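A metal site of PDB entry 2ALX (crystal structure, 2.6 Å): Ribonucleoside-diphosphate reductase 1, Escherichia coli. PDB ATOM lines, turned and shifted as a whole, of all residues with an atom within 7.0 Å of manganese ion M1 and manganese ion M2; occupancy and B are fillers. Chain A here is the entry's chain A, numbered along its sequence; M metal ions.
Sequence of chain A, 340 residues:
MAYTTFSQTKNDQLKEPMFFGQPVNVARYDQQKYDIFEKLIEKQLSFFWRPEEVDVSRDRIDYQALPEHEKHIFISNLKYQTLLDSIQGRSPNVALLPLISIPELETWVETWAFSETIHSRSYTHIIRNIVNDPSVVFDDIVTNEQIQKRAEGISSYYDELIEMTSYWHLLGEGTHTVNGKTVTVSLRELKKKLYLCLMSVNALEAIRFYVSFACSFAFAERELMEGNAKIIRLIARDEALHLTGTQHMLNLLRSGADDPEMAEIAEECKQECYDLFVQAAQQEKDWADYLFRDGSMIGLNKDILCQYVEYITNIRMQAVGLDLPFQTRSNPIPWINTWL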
ATOM      1  N   GLN A  81      24.698   5.762 -32.539  1.00  0.00           N
ATOM      2  CA  GLN A  81      23.836   5.313 -31.451  1.00  0.00           C
ATOM      3  C   GLN A  81      23.423   3.879 -31.731  1.00  0.00           C
ATOM      4  O   GLN A  81      23.446   3.025 -30.840  1.00  0.00           O
ATOM      5  CB  GLN A  81      22.606   6.225 -31.328  1.00  0.00           C
ATOM      6  CG  GLN A  81      22.958   7.708 -31.167  1.00  0.00           C
ATOM      7  CD  GLN A  81      21.770   8.594 -30.789  1.00  0.00           C
ATOM      8  OE1 GLN A  81      20.705   8.525 -31.405  1.00  0.00           O
ATOM      9  NE2 GLN A  81      21.964   9.432 -29.781  1.00  0.00           N
ATOM     10  N   LEU A  84      26.390   1.521 -30.948  1.00  0.00           N
ATOM     11  CA  LEU A  84      26.543   1.333 -29.517  1.00  0.00           C
ATOM     12  C   LEU A  84      25.542   0.349 -28.978  1.00  0.00           C
ATOM     13  O   LEU A  84      25.926  -0.612 -28.317  1.00  0.00           O
ATOM     14  CB  LEU A  84      26.414   2.667 -28.797  1.00  0.00           C
ATOM     15  CG  LEU A  84      27.589   3.635 -28.970  1.00  0.00           C
ATOM     16  CD1 LEU A  84      27.394   4.829 -28.028  1.00  0.00           C
ATOM     17  CD2 LEU A  84      28.889   2.921 -28.645  1.00  0.00           C
ATOM     18  N   ASP A  85      24.257   0.553 -29.258  1.00  0.00           N
ATOM     19  CA  ASP A  85      23.236  -0.337 -28.748  1.00  0.00           C
ATOM     20  C   ASP A  85      23.225  -1.701 -29.432  1.00  0.00           C
ATOM     21  O   ASP A  85      22.696  -2.657 -28.875  1.00  0.00           O
ATOM     22  CB  ASP A  85      21.845   0.304 -28.802  1.00  0.00           C
ATOM     23  CG  ASP A  85      21.585   1.259 -27.623  1.00  0.00           C
ATOM     24  OD1 ASP A  85      22.142   1.032 -26.532  1.00  0.00           O
ATOM     25  OD2 ASP A  85      20.807   2.223 -27.778  1.00  0.00           O
ATOM     26  N   GLN A  88      25.782  -3.180 -27.121  1.00  0.00           N
ATOM     27  CA  GLN A  88      25.196  -3.322 -25.801  1.00  0.00           C
ATOM     28  C   GLN A  88      24.042  -4.284 -25.674  1.00  0.00           C
ATOM     29  O   GLN A  88      23.804  -4.807 -24.595  1.00  0.00           O
ATOM     30  CB  GLN A  88      24.772  -1.962 -25.257  1.00  0.00           C
ATOM     31  CG  GLN A  88      25.924  -1.038 -24.827  1.00  0.00           C
ATOM     32  CD  GLN A  88      26.846  -1.675 -23.805  1.00  0.00           C
ATOM     33  OE1 GLN A  88      27.721  -2.453 -24.148  1.00  0.00           O
ATOM     34  NE2 GLN A  88      26.639  -1.354 -22.531  1.00  0.00           N
ATOM     35  N   TRP A 112      19.016  -5.178 -18.338  1.00  0.00           N
ATOM     36  CA  TRP A 112      19.817  -4.122 -18.937  1.00  0.00           C
ATOM     37  C   TRP A 112      20.049  -4.398 -20.441  1.00  0.00           C
ATOM     38  O   TRP A 112      19.821  -3.525 -21.282  1.00  0.00           O
ATOM     39  CB  TRP A 112      21.132  -4.021 -18.141  1.00  0.00           C
ATOM     40  CG  TRP A 112      22.261  -3.213 -18.776  1.00  0.00           C
ATOM     41  CD1 TRP A 112      22.147  -2.274 -19.769  1.00  0.00           C
ATOM     42  CD2 TRP A 112      23.645  -3.260 -18.415  1.00  0.00           C
ATOM     43  NE1 TRP A 112      23.374  -1.729 -20.044  1.00  0.00           N
ATOM     44  CE2 TRP A 112      24.320  -2.319 -19.235  1.00  0.00           C
ATOM     45  CE3 TRP A 112      24.385  -4.011 -17.489  1.00  0.00           C
ATOM     46  CZ2 TRP A 112      25.707  -2.098 -19.146  1.00  0.00           C
ATOM     47  CZ3 TRP A 112      25.772  -3.790 -17.400  1.00  0.00           C
ATOM     48  CH2 TRP A 112      26.412  -2.836 -18.224  1.00  0.00           C
ATOM     49  N   SER A 115      16.716  -4.056 -22.352  1.00  0.00           N
ATOM     50  CA  SER A 115      16.365  -2.671 -22.673  1.00  0.00           C
ATOM     51  C   SER A 115      17.173  -2.113 -23.852  1.00  0.00           C
ATOM     52  O   SER A 115      16.664  -1.300 -24.620  1.00  0.00           O
ATOM     53  CB  SER A 115      16.489  -1.756 -21.440  1.00  0.00           C
ATOM     54  OG  SER A 115      17.804  -1.724 -20.910  1.00  0.00           O
ATOM     55  N   GLU A 116      18.401  -2.569 -24.036  1.00  0.00           N
ATOM     56  CA  GLU A 116      19.180  -2.059 -25.164  1.00  0.00           C
ATOM     57  C   GLU A 116      18.631  -2.535 -26.499  1.00  0.00           C
ATOM     58  O   GLU A 116      18.800  -1.851 -27.517  1.00  0.00           O
ATOM     59  CB  GLU A 116      20.657  -2.448 -25.028  1.00  0.00           C
ATOM     60  CG  GLU A 116      21.272  -2.006 -23.709  1.00  0.00           C
ATOM     61  CD  GLU A 116      21.503  -0.499 -23.598  1.00  0.00           C
ATOM     62  OE1 GLU A 116      20.818   0.296 -24.275  1.00  0.00           O
ATOM     63  OE2 GLU A 116      22.371  -0.109 -22.783  1.00  0.00           O
ATOM     64  N   THR A 117      17.969  -3.699 -26.526  1.00  0.00           N
ATOM     65  CA  THR A 117      17.414  -4.203 -27.782  1.00  0.00           C
ATOM     66  C   THR A 117      16.207  -3.352 -28.163  1.00  0.00           C
ATOM     67  O   THR A 117      15.912  -3.136 -29.349  1.00  0.00           O
ATOM     68  CB  THR A 117      17.007  -5.709 -27.693  1.00  0.00           C
ATOM     69  OG1 THR A 117      15.900  -5.875 -26.801  1.00  0.00           O
ATOM     70  CG2 THR A 117      18.170  -6.527 -27.202  1.00  0.00           C
ATOM     71  N   HIS A 119      16.026  -0.207 -27.596  1.00  0.00           N
ATOM     72  CA  HIS A 119      16.614   0.997 -28.170  1.00  0.00           C
ATOM     73  C   HIS A 119      16.996   0.701 -29.617  1.00  0.00           C
ATOM     74  O   HIS A 119      16.740   1.508 -30.516  1.00  0.00           O
ATOM     75  CB  HIS A 119      17.860   1.428 -27.380  1.00  0.00           C
ATOM     76  CG  HIS A 119      17.593   1.759 -25.953  1.00  0.00           C
ATOM     77  ND1 HIS A 119      18.601   2.097 -25.067  1.00  0.00           N
ATOM     78  CD2 HIS A 119      16.438   1.815 -25.244  1.00  0.00           C
ATOM     79  CE1 HIS A 119      18.071   2.336 -23.878  1.00  0.00           C
ATOM     80  NE2 HIS A 119      16.760   2.174 -23.963  1.00  0.00           N
ATOM     81  N   SER A 120      17.607  -0.448 -29.877  1.00  0.00           N
ATOM     82  CA  SER A 120      17.978  -0.799 -31.243  1.00  0.00           C
ATOM     83  C   SER A 120      16.730  -0.711 -32.120  1.00  0.00           C
ATOM     84  O   SER A 120      16.757  -0.130 -33.193  1.00  0.00           O
ATOM     85  CB  SER A 120      18.521  -2.219 -31.297  1.00  0.00           C
ATOM     86  OG  SER A 120      19.641  -2.367 -30.450  1.00  0.00           O
ATOM     87  N   TYR A 123      15.713   2.713 -32.979  1.00  0.00           N
ATOM     88  CA  TYR A 123      16.539   3.257 -34.045  1.00  0.00           C
ATOM     89  C   TYR A 123      16.056   2.767 -35.403  1.00  0.00           C
ATOM     90  O   TYR A 123      16.057   3.515 -36.368  1.00  0.00           O
ATOM     91  CB  TYR A 123      18.012   2.858 -33.872  1.00  0.00           C
ATOM     92  CG  TYR A 123      18.647   3.349 -32.599  1.00  0.00           C
ATOM     93  CD1 TYR A 123      18.340   4.622 -32.085  1.00  0.00           C
ATOM     94  CD2 TYR A 123      19.530   2.545 -31.886  1.00  0.00           C
ATOM     95  CE1 TYR A 123      18.908   5.072 -30.904  1.00  0.00           C
ATOM     96  CE2 TYR A 123      20.096   2.981 -30.703  1.00  0.00           C
ATOM     97  CZ  TYR A 123      19.775   4.233 -30.206  1.00  0.00           C
ATOM     98  OH  TYR A 123      20.314   4.660 -29.024  1.00  0.00           O
ATOM     99  N   LEU A 204      31.170   4.135 -21.971  1.00  0.00           N
ATOM    100  CA  LEU A 204      30.269   4.029 -23.104  1.00  0.00           C
ATOM    101  C   LEU A 204      28.862   4.492 -22.727  1.00  0.00           C
ATOM    102  O   LEU A 204      28.184   5.152 -23.517  1.00  0.00           O
ATOM    103  CB  LEU A 204      30.250   2.577 -23.593  1.00  0.00           C
ATOM    104  CG  LEU A 204      29.450   2.245 -24.864  1.00  0.00           C
ATOM    105  CD1 LEU A 204      29.845   0.857 -25.366  1.00  0.00           C
ATOM    106  CD2 LEU A 204      27.973   2.310 -24.547  1.00  0.00           C
ATOM    107  N   GLU A 205      28.433   4.152 -21.522  1.00  0.00           N
ATOM    108  CA  GLU A 205      27.109   4.530 -21.055  1.00  0.00           C
ATOM    109  C   GLU A 205      27.082   5.942 -20.530  1.00  0.00           C
ATOM    110  O   GLU A 205      26.158   6.694 -20.820  1.00  0.00           O
ATOM    111  CB  GLU A 205      26.638   3.575 -19.937  1.00  0.00           C
ATOM    112  CG  GLU A 205      26.547   2.090 -20.316  1.00  0.00           C
ATOM    113  CD  GLU A 205      25.219   1.671 -20.915  1.00  0.00           C
ATOM    114  OE1 GLU A 205      24.284   2.484 -20.974  1.00  0.00           O
ATOM    115  OE2 GLU A 205      25.101   0.503 -21.341  1.00  0.00           O
ATOM    116  N   PHE A 209      27.333   7.832 -24.973  1.00  0.00           N
ATOM    117  CA  PHE A 209      25.924   8.082 -25.219  1.00  0.00           C
ATOM    118  C   PHE A 209      25.451   9.508 -24.975  1.00  0.00           C
ATOM    119  O   PHE A 209      24.614  10.005 -25.728  1.00  0.00           O
ATOM    120  CB  PHE A 209      25.065   7.130 -24.401  1.00  0.00           C
ATOM    121  CG  PHE A 209      24.618   5.948 -25.182  1.00  0.00           C
ATOM    122  CD1 PHE A 209      23.765   6.098 -26.258  1.00  0.00           C
ATOM    123  CD2 PHE A 209      25.126   4.689 -24.907  1.00  0.00           C
ATOM    124  CE1 PHE A 209      23.421   5.027 -27.051  1.00  0.00           C
ATOM    125  CE2 PHE A 209      24.788   3.602 -25.703  1.00  0.00           C
ATOM    126  CZ  PHE A 209      23.926   3.776 -26.782  1.00  0.00           C
ATOM    127  N   PHE A 213      23.377  12.527 -27.205  1.00  0.00           N
ATOM    128  CA  PHE A 213      22.099  13.150 -26.873  1.00  0.00           C
ATOM    129  C   PHE A 213      22.177  14.655 -27.050  1.00  0.00           C
ATOM    130  O   PHE A 213      21.166  15.317 -27.312  1.00  0.00           O
ATOM    131  CB  PHE A 213      21.702  12.858 -25.422  1.00  0.00           C
ATOM    132  CG  PHE A 213      21.610  11.406 -25.095  1.00  0.00           C
ATOM    133  CD1 PHE A 213      21.229  10.483 -26.063  1.00  0.00           C
ATOM    134  CD2 PHE A 213      21.878  10.954 -23.803  1.00  0.00           C
ATOM    135  CE1 PHE A 213      21.119   9.119 -25.758  1.00  0.00           C
ATOM    136  CE2 PHE A 213      21.770   9.605 -23.482  1.00  0.00           C
ATOM    137  CZ  PHE A 213      21.382   8.682 -24.462  1.00  0.00           C
ATOM    138  N   ILE A 235      15.292   6.784 -24.121  1.00  0.00           N
ATOM    139  CA  ILE A 235      16.559   6.031 -24.108  1.00  0.00           C
ATOM    140  C   ILE A 235      17.498   6.608 -23.036  1.00  0.00           C
ATOM    141  O   ILE A 235      18.154   5.866 -22.308  1.00  0.00           O
ATOM    142  CB  ILE A 235      17.270   6.065 -25.497  1.00  0.00           C
ATOM    143  CG1 ILE A 235      16.439   5.321 -26.544  1.00  0.00           C
ATOM    144  CG2 ILE A 235      18.620   5.413 -25.408  1.00  0.00           C
ATOM    145  CD1 ILE A 235      16.969   5.436 -27.946  1.00  0.00           C
ATOM    146  N   ASP A 238      16.837   5.519 -19.604  1.00  0.00           N
ATOM    147  CA  ASP A 238      17.373   4.169 -19.404  1.00  0.00           C
ATOM    148  C   ASP A 238      18.886   4.147 -19.213  1.00  0.00           C
ATOM    149  O   ASP A 238      19.391   3.501 -18.300  1.00  0.00           O
ATOM    150  CB  ASP A 238      17.059   3.256 -20.579  1.00  0.00           C
ATOM    151  CG  ASP A 238      15.611   2.894 -20.673  1.00  0.00           C
ATOM    152  OD1 ASP A 238      14.960   2.772 -19.621  1.00  0.00           O
ATOM    153  OD2 ASP A 238      15.135   2.720 -21.810  1.00  0.00           O
ATOM    154  N   GLU A 239      19.592   4.845 -20.104  1.00  0.00           N
ATOM    155  CA  GLU A 239      21.052   4.850 -20.028  1.00  0.00           C
ATOM    156  C   GLU A 239      21.468   5.401 -18.686  1.00  0.00           C
ATOM    157  O   GLU A 239      22.565   5.149 -18.208  1.00  0.00           O
ATOM    158  CB  GLU A 239      21.653   5.678 -21.178  1.00  0.00           C
ATOM    159  CG  GLU A 239      21.143   5.345 -22.601  1.00  0.00           C
ATOM    160  CD  GLU A 239      21.490   3.944 -23.098  1.00  0.00           C
ATOM    161  OE1 GLU A 239      22.203   3.190 -22.389  1.00  0.00           O
ATOM    162  OE2 GLU A 239      21.063   3.576 -24.217  1.00  0.00           O
ATOM    163  N   ALA A 240      20.569   6.148 -18.038  1.00  0.00           N
ATOM    164  CA  ALA A 240      20.865   6.696 -16.714  1.00  0.00           C
ATOM    165  C   ALA A 240      20.834   5.538 -15.718  1.00  0.00           C
ATOM    166  O   ALA A 240      21.680   5.458 -14.818  1.00  0.00           O
ATOM    167  CB  ALA A 240      19.850   7.747 -16.333  1.00  0.00           C
ATOM    168  N   HIS A 242      21.438   2.460 -16.461  1.00  0.00           N
ATOM    169  CA  HIS A 242      22.601   1.681 -16.823  1.00  0.00           C
ATOM    170  C   HIS A 242      23.884   2.223 -16.228  1.00  0.00           C
ATOM    171  O   HIS A 242      24.658   1.453 -15.647  1.00  0.00           O
ATOM    172  CB  HIS A 242      22.732   1.594 -18.347  1.00  0.00           C
ATOM    173  CG  HIS A 242      21.532   1.015 -19.026  1.00  0.00           C
ATOM    174  ND1 HIS A 242      21.375   1.029 -20.398  1.00  0.00           N
ATOM    175  CD2 HIS A 242      20.428   0.413 -18.528  1.00  0.00           C
ATOM    176  CE1 HIS A 242      20.225   0.463 -20.709  1.00  0.00           C
ATOM    177  NE2 HIS A 242      19.623   0.087 -19.597  1.00  0.00           N
ATOM    178  N   LEU A 243      24.129   3.517 -16.343  1.00  0.00           N
ATOM    179  CA  LEU A 243      25.341   4.090 -15.779  1.00  0.00           C
ATOM    180  C   LEU A 243      25.317   4.007 -14.247  1.00  0.00           C
ATOM    181  O   LEU A 243      26.369   3.930 -13.616  1.00  0.00           O
ATOM    182  CB  LEU A 243      25.550   5.536 -16.244  1.00  0.00           C
ATOM    183  CG  LEU A 243      24.697   6.672 -15.671  1.00  0.00           C
ATOM    184  CD1 LEU A 243      25.178   7.044 -14.271  1.00  0.00           C
ATOM    185  CD2 LEU A 243      24.806   7.881 -16.599  1.00  0.00           C
HETATM  186 MN    MN M   1      20.843   1.934 -25.173  1.00  0.00          MN
HETATM  187 MN    MN M   2      22.865   1.450 -21.971  1.00  0.00          MN
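Manganese ion M1 is bound by OE1 of Glu 116, at 1.9 Å. OE2 of Glu 239 binds manganese ion M1 (1.9 Å). Manganese ion M1 is bound by OD1 of Asp 85. Manganese ion M1 is bound by ND1 of His 119 (2.3 Å). Manganese ion M1 is bound by OD2 of Asp 85 (2.6 Å).
Phe 209 touches manganese ion M1. Five residues have an atom within 4 Å of manganese ion M1: Asp 85, Glu 116, His 119, Phe 209 and Glu 239. Along chain A the residues within 4 Å of manganese ion M1 span positions 85 to 239.
OE2 of Glu 116 binds manganese ion M2 (1.8 Å). OE1 of Glu 239 is bound to manganese ion M2 (1.9 Å). OE1 of Glu 205 is bound to manganese ion M2 (2.0 Å). ND1 of His 242 binds manganese ion M2, 2.2 Å away. Manganese ion M2 is bound by the side-chain carboxylate (OE2) of Glu 205 (2.5 Å). Manganese ion M2 has five donor atoms within binding distance.
Trp 112 touches manganese ion M2 (NE1 to MN, 3.8 Å). Within 4 Å of manganese ion M2: Trp 112, Glu 116, Glu 205, Glu 239 and His 242. The nearest printed residue that does not touch manganese ion M2 is Asp 85 (4.6 Å).
The side-chain hydroxyl of Tyr 123 sits close to the side-chain carboxylate of Asp 85 (2.8 Å). The side-chain carboxylate of Glu 205 lies close to the indole nitrogen of Trp 112 (3.1 Å). O of Asp 85 sits at hydrogen-bond distance from OG of Ser 120. The backbone NH of Phe 209 is in hydrogen-bond range of the backbone carbonyl oxygen of Leu 204, at 3.2 Å. O of Trp 112 sits at hydrogen-bond distance from OG of Ser 115, at 2.7 Å. The indole nitrogen (NE1) of Trp 112 lies close to the side-chain carboxylate (OE2) of Glu 116. NE2 of His 242 lies within hydrogen-bond range of OG of Ser 115. The indole nitrogen (NE1) of Trp 112 lies close to a ring nitrogen (ND1) of His 242 (3.4 Å).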
